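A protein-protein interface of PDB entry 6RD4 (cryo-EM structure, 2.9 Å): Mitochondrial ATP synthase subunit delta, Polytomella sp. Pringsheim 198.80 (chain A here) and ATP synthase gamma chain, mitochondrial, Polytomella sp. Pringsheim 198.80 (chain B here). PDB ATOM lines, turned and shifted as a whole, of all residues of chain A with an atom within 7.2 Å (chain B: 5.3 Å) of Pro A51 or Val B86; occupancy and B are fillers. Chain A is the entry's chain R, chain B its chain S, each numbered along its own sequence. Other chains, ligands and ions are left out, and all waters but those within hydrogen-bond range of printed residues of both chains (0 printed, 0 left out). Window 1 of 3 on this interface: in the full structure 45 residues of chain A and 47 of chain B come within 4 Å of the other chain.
Of the 11 printed residues of chain A, 7 touch a printed residue of chain B. Printed residues of chain A that touch a printed residue of chain B: Glu A49, Phe A50, Pro A51, Ser A52, Thr A55, Val A57 and His A137. Hydrophobic or aromatic side chains of chain A that line the printed part of chain B: Phe A50, Pro A51, Val A57 and His A137. Of the 14 printed residues of chain B, 7 touch a printed residue of chain A. Among the printed residues, 16 pairs touch across the chains.
O of Thr A55 sits at hydrogen-bond distance from NZ of Lys A58 (3.0 Å). The side-chain hydroxyl (OG1) of Thr A55 sits at hydrogen-bond distance from the backbone carbonyl oxygen (O) of Val A57. N of Phe A50 sits at hydrogen-bond distance from OD1 of Asn A53 (2.8 Å). OD1 of Asn A53 lies close to OE1 of Glu A49 (3.3 Å).
Among the printed residues, merely in contact across the chains: Glu A49 with Thr B206 (3.3 Å), Phe A50 with Asp B91 (3.6 Å), Phe A50 with Thr B206 (3.96 Å), Phe A50 with Val B207 (3.8 Å), Pro A51 with Val B86 (3.8 Å), Pro A51 with Thr B206 (3.9 Å), Pro A51 with Val B207 (3.6 Å), Thr A55 with Asp B83 (3.4 Å), Thr A55 with Val B86 (3.7 Å), His A137 with Arg B87 (3.8 Å) and His A137 with Leu B88 (3.7 Å).
The backbone carbonyl oxygen of Val A57 sits at hydrogen-bond distance from the guanidinium group of Arg B87 (3.1 Å). The backbone carbonyl oxygen of Glu A49 is in hydrogen-bond range of the backbone NH of Val B207 (3.1 Å). The side-chain carboxylate (OD1) of Asp B91 lies close to the backbone nitrogen (N) of Pro A51 (3.5 Å). The side-chain hydroxyl (OG1) of Thr A55 is in hydrogen-bond range of the guanidinium group (NH1) of Arg B87, 3.3 Å away. The side-chain carboxylate of Asp B91 lies within hydrogen-bond range of the backbone NH of Ser A52 (3.2 Å).
Printed residues of chain B within 4 Å of Phe A50: Asp B91 (3.6 Å), Thr B206 (3.96 Å) and Val B207 (3.8 Å). Of chain B, only Val B86 (3.8 Å), Asp B91 (3.3 Å), Thr B206 (3.9 Å) and Val B207 (3.6 Å) come within 4 Å of Pro A51. Printed residues of chain A within 4 Å of Asp B83: Thr A55. Val B86 touches just these residues of chain A: Pro A51 (3.8 Å) and Thr A55 (3.7 Å). The nearest residue of chain B that does not touch Pro A51 is Ala B208 (4.2 Å).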
ATOM      1  N   GLU A  49      34.008  -8.588 -23.526  1.00  0.00           N
ATOM      2  CA  GLU A  49      32.723  -8.518 -22.865  1.00  0.00           C
ATOM      3  C   GLU A  49      32.551  -9.720 -21.946  1.00  0.00           C
ATOM      4  O   GLU A  49      33.333 -10.671 -21.966  1.00  0.00           O
ATOM      5  CB  GLU A  49      31.601  -8.458 -23.886  1.00  0.00           C
ATOM      6  CG  GLU A  49      31.631  -7.219 -24.730  1.00  0.00           C
ATOM      7  CD  GLU A  49      31.173  -5.986 -23.993  1.00  0.00           C
ATOM      8  OE1 GLU A  49      30.352  -6.111 -23.064  1.00  0.00           O
ATOM      9  OE2 GLU A  49      31.646  -4.885 -24.337  1.00  0.00           O
ATOM     10  N   PHE A  50      31.526  -9.651 -21.110  1.00  0.00           N
ATOM     11  CA  PHE A  50      31.214 -10.689 -20.145  1.00  0.00           C
ATOM     12  C   PHE A  50      29.725 -10.971 -20.191  1.00  0.00           C
ATOM     13  O   PHE A  50      28.942 -10.091 -20.557  1.00  0.00           O
ATOM     14  CB  PHE A  50      31.624 -10.262 -18.733  1.00  0.00           C
ATOM     15  CG  PHE A  50      32.983  -9.663 -18.664  1.00  0.00           C
ATOM     16  CD1 PHE A  50      33.143  -8.295 -18.586  1.00  0.00           C
ATOM     17  CD2 PHE A  50      34.103 -10.468 -18.689  1.00  0.00           C
ATOM     18  CE1 PHE A  50      34.397  -7.741 -18.531  1.00  0.00           C
ATOM     19  CE2 PHE A  50      35.357  -9.920 -18.631  1.00  0.00           C
ATOM     20  CZ  PHE A  50      35.501  -8.554 -18.557  1.00  0.00           C
ATOM     21  N   PRO A  51      29.300 -12.189 -19.839  1.00  0.00           N
ATOM     22  CA  PRO A  51      27.861 -12.497 -19.858  1.00  0.00           C
ATOM     23  C   PRO A  51      27.032 -11.736 -18.831  1.00  0.00           C
ATOM     24  O   PRO A  51      25.799 -11.760 -18.932  1.00  0.00           O
ATOM     25  CB  PRO A  51      27.820 -14.005 -19.598  1.00  0.00           C
ATOM     26  CG  PRO A  51      29.182 -14.365 -19.116  1.00  0.00           C
ATOM     27  CD  PRO A  51      30.117 -13.406 -19.717  1.00  0.00           C
ATOM     28  N   SER A  52      27.649 -11.045 -17.872  1.00  0.00           N
ATOM     29  CA  SER A  52      26.895 -10.150 -17.005  1.00  0.00           C
ATOM     30  C   SER A  52      26.443  -8.888 -17.719  1.00  0.00           C
ATOM     31  O   SER A  52      25.540  -8.206 -17.227  1.00  0.00           O
ATOM     32  CB  SER A  52      27.723  -9.765 -15.789  1.00  0.00           C
ATOM     33  OG  SER A  52      27.869 -10.870 -14.937  1.00  0.00           O
ATOM     34  N   ASN A  53      27.048  -8.556 -18.850  1.00  0.00           N
ATOM     35  CA  ASN A  53      26.687  -7.349 -19.573  1.00  0.00           C
ATOM     36  C   ASN A  53      25.496  -7.557 -20.491  1.00  0.00           C
ATOM     37  O   ASN A  53      25.074  -6.609 -21.158  1.00  0.00           O
ATOM     38  CB  ASN A  53      27.886  -6.847 -20.376  1.00  0.00           C
ATOM     39  CG  ASN A  53      29.163  -6.866 -19.569  1.00  0.00           C
ATOM     40  OD1 ASN A  53      30.169  -7.428 -19.993  1.00  0.00           O
ATOM     41  ND2 ASN A  53      29.126  -6.262 -18.393  1.00  0.00           N
ATOM     42  N   TYR A  54      24.939  -8.761 -20.539  1.00  0.00           N
ATOM     43  CA  TYR A  54      23.835  -9.056 -21.435  1.00  0.00           C
ATOM     44  C   TYR A  54      22.558  -9.448 -20.717  1.00  0.00           C
ATOM     45  O   TYR A  54      21.513  -9.560 -21.362  1.00  0.00           O
ATOM     46  CB  TYR A  54      24.242 -10.158 -22.408  1.00  0.00           C
ATOM     47  CG  TYR A  54      25.466  -9.778 -23.186  1.00  0.00           C
ATOM     48  CD1 TYR A  54      25.385  -8.838 -24.201  1.00  0.00           C
ATOM     49  CD2 TYR A  54      26.706 -10.333 -22.896  1.00  0.00           C
ATOM     50  CE1 TYR A  54      26.491  -8.471 -24.908  1.00  0.00           C
ATOM     51  CE2 TYR A  54      27.823  -9.968 -23.610  1.00  0.00           C
ATOM     52  CZ  TYR A  54      27.698  -9.036 -24.615  1.00  0.00           C
ATOM     53  OH  TYR A  54      28.770  -8.647 -25.355  1.00  0.00           O
ATOM     54  N   THR A  55      22.600  -9.653 -19.412  1.00  0.00           N
ATOM     55  CA  THR A  55      21.387  -9.885 -18.646  1.00  0.00           C
ATOM     56  C   THR A  55      21.143  -8.712 -17.707  1.00  0.00           C
ATOM     57  O   THR A  55      22.069  -8.201 -17.069  1.00  0.00           O
ATOM     58  CB  THR A  55      21.456 -11.210 -17.879  1.00  0.00           C
ATOM     59  OG1 THR A  55      20.346 -11.309 -16.982  1.00  0.00           O
ATOM     60  CG2 THR A  55      22.755 -11.345 -17.114  1.00  0.00           C
ATOM     61  N   ALA A  56      19.895  -8.249 -17.680  1.00  0.00           N
ATOM     62  CA  ALA A  56      19.506  -7.139 -16.828  1.00  0.00           C
ATOM     63  C   ALA A  56      18.847  -7.595 -15.538  1.00  0.00           C
ATOM     64  O   ALA A  56      18.720  -6.792 -14.608  1.00  0.00           O
ATOM     65  CB  ALA A  56      18.559  -6.200 -17.578  1.00  0.00           C
ATOM     66  N   VAL A  57      18.459  -8.861 -15.454  1.00  0.00           N
ATOM     67  CA  VAL A  57      17.750  -9.411 -14.311  1.00  0.00           C
ATOM     68  C   VAL A  57      18.765 -10.086 -13.406  1.00  0.00           C
ATOM     69  O   VAL A  57      19.514 -10.960 -13.851  1.00  0.00           O
ATOM     70  CB  VAL A  57      16.669 -10.405 -14.762  1.00  0.00           C
ATOM     71  CG1 VAL A  57      15.704 -10.693 -13.628  1.00  0.00           C
ATOM     72  CG2 VAL A  57      15.947  -9.863 -15.989  1.00  0.00           C
ATOM     73  N   LYS A  58      18.802  -9.678 -12.152  1.00  0.00           N
ATOM     74  CA  LYS A  58      19.724 -10.276 -11.208  1.00  0.00           C
ATOM     75  C   LYS A  58      18.953 -11.106 -10.181  1.00  0.00           C
ATOM     76  O   LYS A  58      17.729 -11.253 -10.253  1.00  0.00           O
ATOM     77  CB  LYS A  58      20.584  -9.194 -10.557  1.00  0.00           C
ATOM     78  CG  LYS A  58      21.280  -8.269 -11.541  1.00  0.00           C
ATOM     79  CD  LYS A  58      22.096  -9.043 -12.566  1.00  0.00           C
ATOM     80  CE  LYS A  58      22.752  -8.111 -13.566  1.00  0.00           C
ATOM     81  NZ  LYS A  58      21.771  -7.255 -14.266  1.00  0.00           N
ATOM     82  N   HIS A 137      15.082 -17.488  -7.472  1.00  0.00           N
ATOM     83  CA  HIS A 137      16.055 -16.519  -7.007  1.00  0.00           C
ATOM     84  C   HIS A 137      15.439 -15.665  -5.913  1.00  0.00           C
ATOM     85  O   HIS A 137      14.215 -15.643  -5.767  1.00  0.00           O
ATOM     86  CB  HIS A 137      16.526 -15.686  -8.197  1.00  0.00           C
ATOM     87  CG  HIS A 137      17.453 -16.430  -9.095  1.00  0.00           C
ATOM     88  ND1 HIS A 137      17.061 -16.966 -10.301  1.00  0.00           N
ATOM     89  CD2 HIS A 137      18.749 -16.781  -8.934  1.00  0.00           C
ATOM     90  CE1 HIS A 137      18.082 -17.591 -10.854  1.00  0.00           C
ATOM     91  NE2 HIS A 137      19.121 -17.490 -10.047  1.00  0.00           N
ATOM     92  N   VAL B  82      21.964 -19.163 -20.814  1.00  0.00           N
ATOM     93  CA  VAL B  82      23.179 -18.726 -20.132  1.00  0.00           C
ATOM     94  C   VAL B  82      22.891 -17.715 -19.039  1.00  0.00           C
ATOM     95  O   VAL B  82      23.748 -17.496 -18.181  1.00  0.00           O
ATOM     96  CB  VAL B  82      24.213 -18.132 -21.107  1.00  0.00           C
ATOM     97  CG1 VAL B  82      24.457 -19.075 -22.247  1.00  0.00           C
ATOM     98  CG2 VAL B  82      23.775 -16.788 -21.626  1.00  0.00           C
ATOM     99  N   ASP B  83      21.703 -17.120 -19.028  1.00  0.00           N
ATOM    100  CA  ASP B  83      21.339 -16.075 -18.076  1.00  0.00           C
ATOM    101  C   ASP B  83      21.126 -16.565 -16.637  1.00  0.00           C
ATOM    102  O   ASP B  83      21.584 -15.873 -15.723  1.00  0.00           O
ATOM    103  CB  ASP B  83      20.096 -15.327 -18.570  1.00  0.00           C
ATOM    104  CG  ASP B  83      20.368 -14.484 -19.793  1.00  0.00           C
ATOM    105  OD1 ASP B  83      21.492 -13.957 -19.913  1.00  0.00           O
ATOM    106  OD2 ASP B  83      19.459 -14.357 -20.643  1.00  0.00           O
ATOM    107  N   PRO B  84      20.457 -17.700 -16.355  1.00  0.00           N
ATOM    108  CA  PRO B  84      20.352 -18.107 -14.946  1.00  0.00           C
ATOM    109  C   PRO B  84      21.659 -18.527 -14.311  1.00  0.00           C
ATOM    110  O   PRO B  84      21.838 -18.318 -13.109  1.00  0.00           O
ATOM    111  CB  PRO B  84      19.359 -19.270 -14.996  1.00  0.00           C
ATOM    112  CG  PRO B  84      19.385 -19.697 -16.341  1.00  0.00           C
ATOM    113  CD  PRO B  84      19.509 -18.505 -17.139  1.00  0.00           C
ATOM    114  N   PHE B  85      22.583 -19.104 -15.065  1.00  0.00           N
ATOM    115  CA  PHE B  85      23.831 -19.517 -14.451  1.00  0.00           C
ATOM    116  C   PHE B  85      24.758 -18.351 -14.164  1.00  0.00           C
ATOM    117  O   PHE B  85      25.690 -18.503 -13.371  1.00  0.00           O
ATOM    118  CB  PHE B  85      24.552 -20.504 -15.338  1.00  0.00           C
ATOM    119  CG  PHE B  85      23.822 -21.769 -15.543  1.00  0.00           C
ATOM    120  CD1 PHE B  85      23.854 -22.756 -14.590  1.00  0.00           C
ATOM    121  CD2 PHE B  85      23.105 -21.980 -16.696  1.00  0.00           C
ATOM    122  CE1 PHE B  85      23.180 -23.923 -14.788  1.00  0.00           C
ATOM    123  CE2 PHE B  85      22.431 -23.151 -16.894  1.00  0.00           C
ATOM    124  CZ  PHE B  85      22.465 -24.114 -15.942  1.00  0.00           C
ATOM    125  N   VAL B  86      24.559 -17.202 -14.806  1.00  0.00           N
ATOM    126  CA  VAL B  86      25.375 -16.048 -14.455  1.00  0.00           C
ATOM    127  C   VAL B  86      24.726 -15.200 -13.378  1.00  0.00           C
ATOM    128  O   VAL B  86      25.372 -14.279 -12.863  1.00  0.00           O
ATOM    129  CB  VAL B  86      25.712 -15.154 -15.660  1.00  0.00           C
ATOM    130  CG1 VAL B  86      26.340 -15.970 -16.765  1.00  0.00           C
ATOM    131  CG2 VAL B  86      24.493 -14.432 -16.145  1.00  0.00           C
ATOM    132  N   ARG B  87      23.470 -15.460 -13.031  1.00  0.00           N
ATOM    133  CA  ARG B  87      22.924 -14.829 -11.844  1.00  0.00           C
ATOM    134  C   ARG B  87      22.847 -15.778 -10.665  1.00  0.00           C
ATOM    135  O   ARG B  87      22.619 -15.323  -9.541  1.00  0.00           O
ATOM    136  CB  ARG B  87      21.546 -14.220 -12.114  1.00  0.00           C
ATOM    137  CG  ARG B  87      20.512 -15.117 -12.692  1.00  0.00           C
ATOM    138  CD  ARG B  87      19.219 -14.351 -12.727  1.00  0.00           C
ATOM    139  NE  ARG B  87      18.199 -14.967 -13.558  1.00  0.00           N
ATOM    140  CZ  ARG B  87      17.887 -14.545 -14.772  1.00  0.00           C
ATOM    141  NH1 ARG B  87      18.531 -13.514 -15.288  1.00  0.00           N
ATOM    142  NH2 ARG B  87      16.940 -15.150 -15.467  1.00  0.00           N
ATOM    143  N   LEU B  88      23.047 -17.072 -10.886  1.00  0.00           N
ATOM    144  CA  LEU B  88      23.186 -17.991  -9.767  1.00  0.00           C
ATOM    145  C   LEU B  88      24.627 -18.037  -9.290  1.00  0.00           C
ATOM    146  O   LEU B  88      24.900 -17.909  -8.095  1.00  0.00           O
ATOM    147  CB  LEU B  88      22.720 -19.387 -10.166  1.00  0.00           C
ATOM    148  CG  LEU B  88      22.488 -20.359  -9.022  1.00  0.00           C
ATOM    149  CD1 LEU B  88      21.308 -19.883  -8.239  1.00  0.00           C
ATOM    150  CD2 LEU B  88      22.228 -21.737  -9.555  1.00  0.00           C
ATOM    151  N   PHE B  89      25.560 -18.204 -10.219  1.00  0.00           N
ATOM    152  CA  PHE B  89      26.971 -18.350  -9.910  1.00  0.00           C
ATOM    153  C   PHE B  89      27.759 -17.074 -10.118  1.00  0.00           C
ATOM    154  O   PHE B  89      28.951 -17.049  -9.812  1.00  0.00           O
ATOM    155  CB  PHE B  89      27.574 -19.450 -10.772  1.00  0.00           C
ATOM    156  CG  PHE B  89      27.127 -20.810 -10.395  1.00  0.00           C
ATOM    157  CD1 PHE B  89      26.790 -21.100  -9.094  1.00  0.00           C
ATOM    158  CD2 PHE B  89      27.034 -21.800 -11.347  1.00  0.00           C
ATOM    159  CE1 PHE B  89      26.372 -22.354  -8.749  1.00  0.00           C
ATOM    160  CE2 PHE B  89      26.620 -23.058 -11.005  1.00  0.00           C
ATOM    161  CZ  PHE B  89      26.293 -23.334  -9.705  1.00  0.00           C
ATOM    162  N   GLY B  90      27.139 -16.031 -10.652  1.00  0.00           N
ATOM    163  CA  GLY B  90      27.876 -14.814 -10.882  1.00  0.00           C
ATOM    164  C   GLY B  90      28.802 -14.901 -12.086  1.00  0.00           C
ATOM    165  O   GLY B  90      28.639 -15.723 -12.988  1.00  0.00           O
ATOM    166  N   ASP B  91      29.801 -14.023 -12.075  1.00  0.00           N
ATOM    167  CA  ASP B  91      30.735 -13.882 -13.189  1.00  0.00           C
ATOM    168  C   ASP B  91      32.079 -13.474 -12.615  1.00  0.00           C
ATOM    169  O   ASP B  91      32.244 -12.328 -12.195  1.00  0.00           O
ATOM    170  CB  ASP B  91      30.243 -12.834 -14.163  1.00  0.00           C
ATOM    171  CG  ASP B  91      30.719 -13.065 -15.563  1.00  0.00           C
ATOM    172  OD1 ASP B  91      30.018 -12.600 -16.480  1.00  0.00           O
ATOM    173  OD2 ASP B  91      31.774 -13.702 -15.752  1.00  0.00           O
ATOM    174  N   THR B 206      33.927 -12.260 -26.060  1.00  0.00           N
ATOM    175  CA  THR B 206      33.499 -12.523 -24.703  1.00  0.00           C
ATOM    176  C   THR B 206      34.455 -13.513 -24.067  1.00  0.00           C
ATOM    177  O   THR B 206      34.966 -14.414 -24.736  1.00  0.00           O
ATOM    178  CB  THR B 206      32.075 -13.070 -24.693  1.00  0.00           C
ATOM    179  OG1 THR B 206      31.251 -12.241 -25.511  1.00  0.00           O
ATOM    180  CG2 THR B 206      31.491 -13.066 -23.299  1.00  0.00           C
ATOM    181  N   VAL B 207      34.735 -13.302 -22.788  1.00  0.00           N
ATOM    182  CA  VAL B 207      35.294 -14.324 -21.922  1.00  0.00           C
ATOM    183  C   VAL B 207      34.192 -14.762 -20.975  1.00  0.00           C
ATOM    184  O   VAL B 207      33.650 -13.951 -20.217  1.00  0.00           O
ATOM    185  CB  VAL B 207      36.506 -13.801 -21.138  1.00  0.00           C
ATOM    186  CG1 VAL B 207      37.072 -14.893 -20.269  1.00  0.00           C
ATOM    187  CG2 VAL B 207      37.533 -13.270 -22.075  1.00  0.00           C
ATOM    188  N   ALA B 208      33.863 -16.044 -21.012  1.00  0.00           N
ATOM    189  CA  ALA B 208      32.842 -16.599 -20.143  1.00  0.00           C
ATOM    190  C   ALA B 208      33.513 -17.629 -19.265  1.00  0.00           C
ATOM    191  O   ALA B 208      34.143 -18.560 -19.770  1.00  0.00           O
ATOM    192  CB  ALA B 208      31.702 -17.227 -20.938  1.00  0.00           C
ATOM    193  N   HIS B 250      26.528 -25.897 -16.464  1.00  0.00           N
ATOM    194  CA  HIS B 250      26.891 -24.527 -16.798  1.00  0.00           C
ATOM    195  C   HIS B 250      28.038 -24.495 -17.789  1.00  0.00           C
ATOM    196  O   HIS B 250      28.161 -23.547 -18.565  1.00  0.00           O
ATOM    197  CB  HIS B 250      27.232 -23.755 -15.532  1.00  0.00           C
ATOM    198  CG  HIS B 250      27.755 -22.377 -15.772  1.00  0.00           C
ATOM    199  ND1 HIS B 250      27.282 -21.570 -16.777  1.00  0.00           N
ATOM    200  CD2 HIS B 250      28.614 -21.618 -15.056  1.00  0.00           C
ATOM    201  CE1 HIS B 250      27.880 -20.395 -16.715  1.00  0.00           C
ATOM    202  NE2 HIS B 250      28.694 -20.398 -15.678  1.00  0.00           N
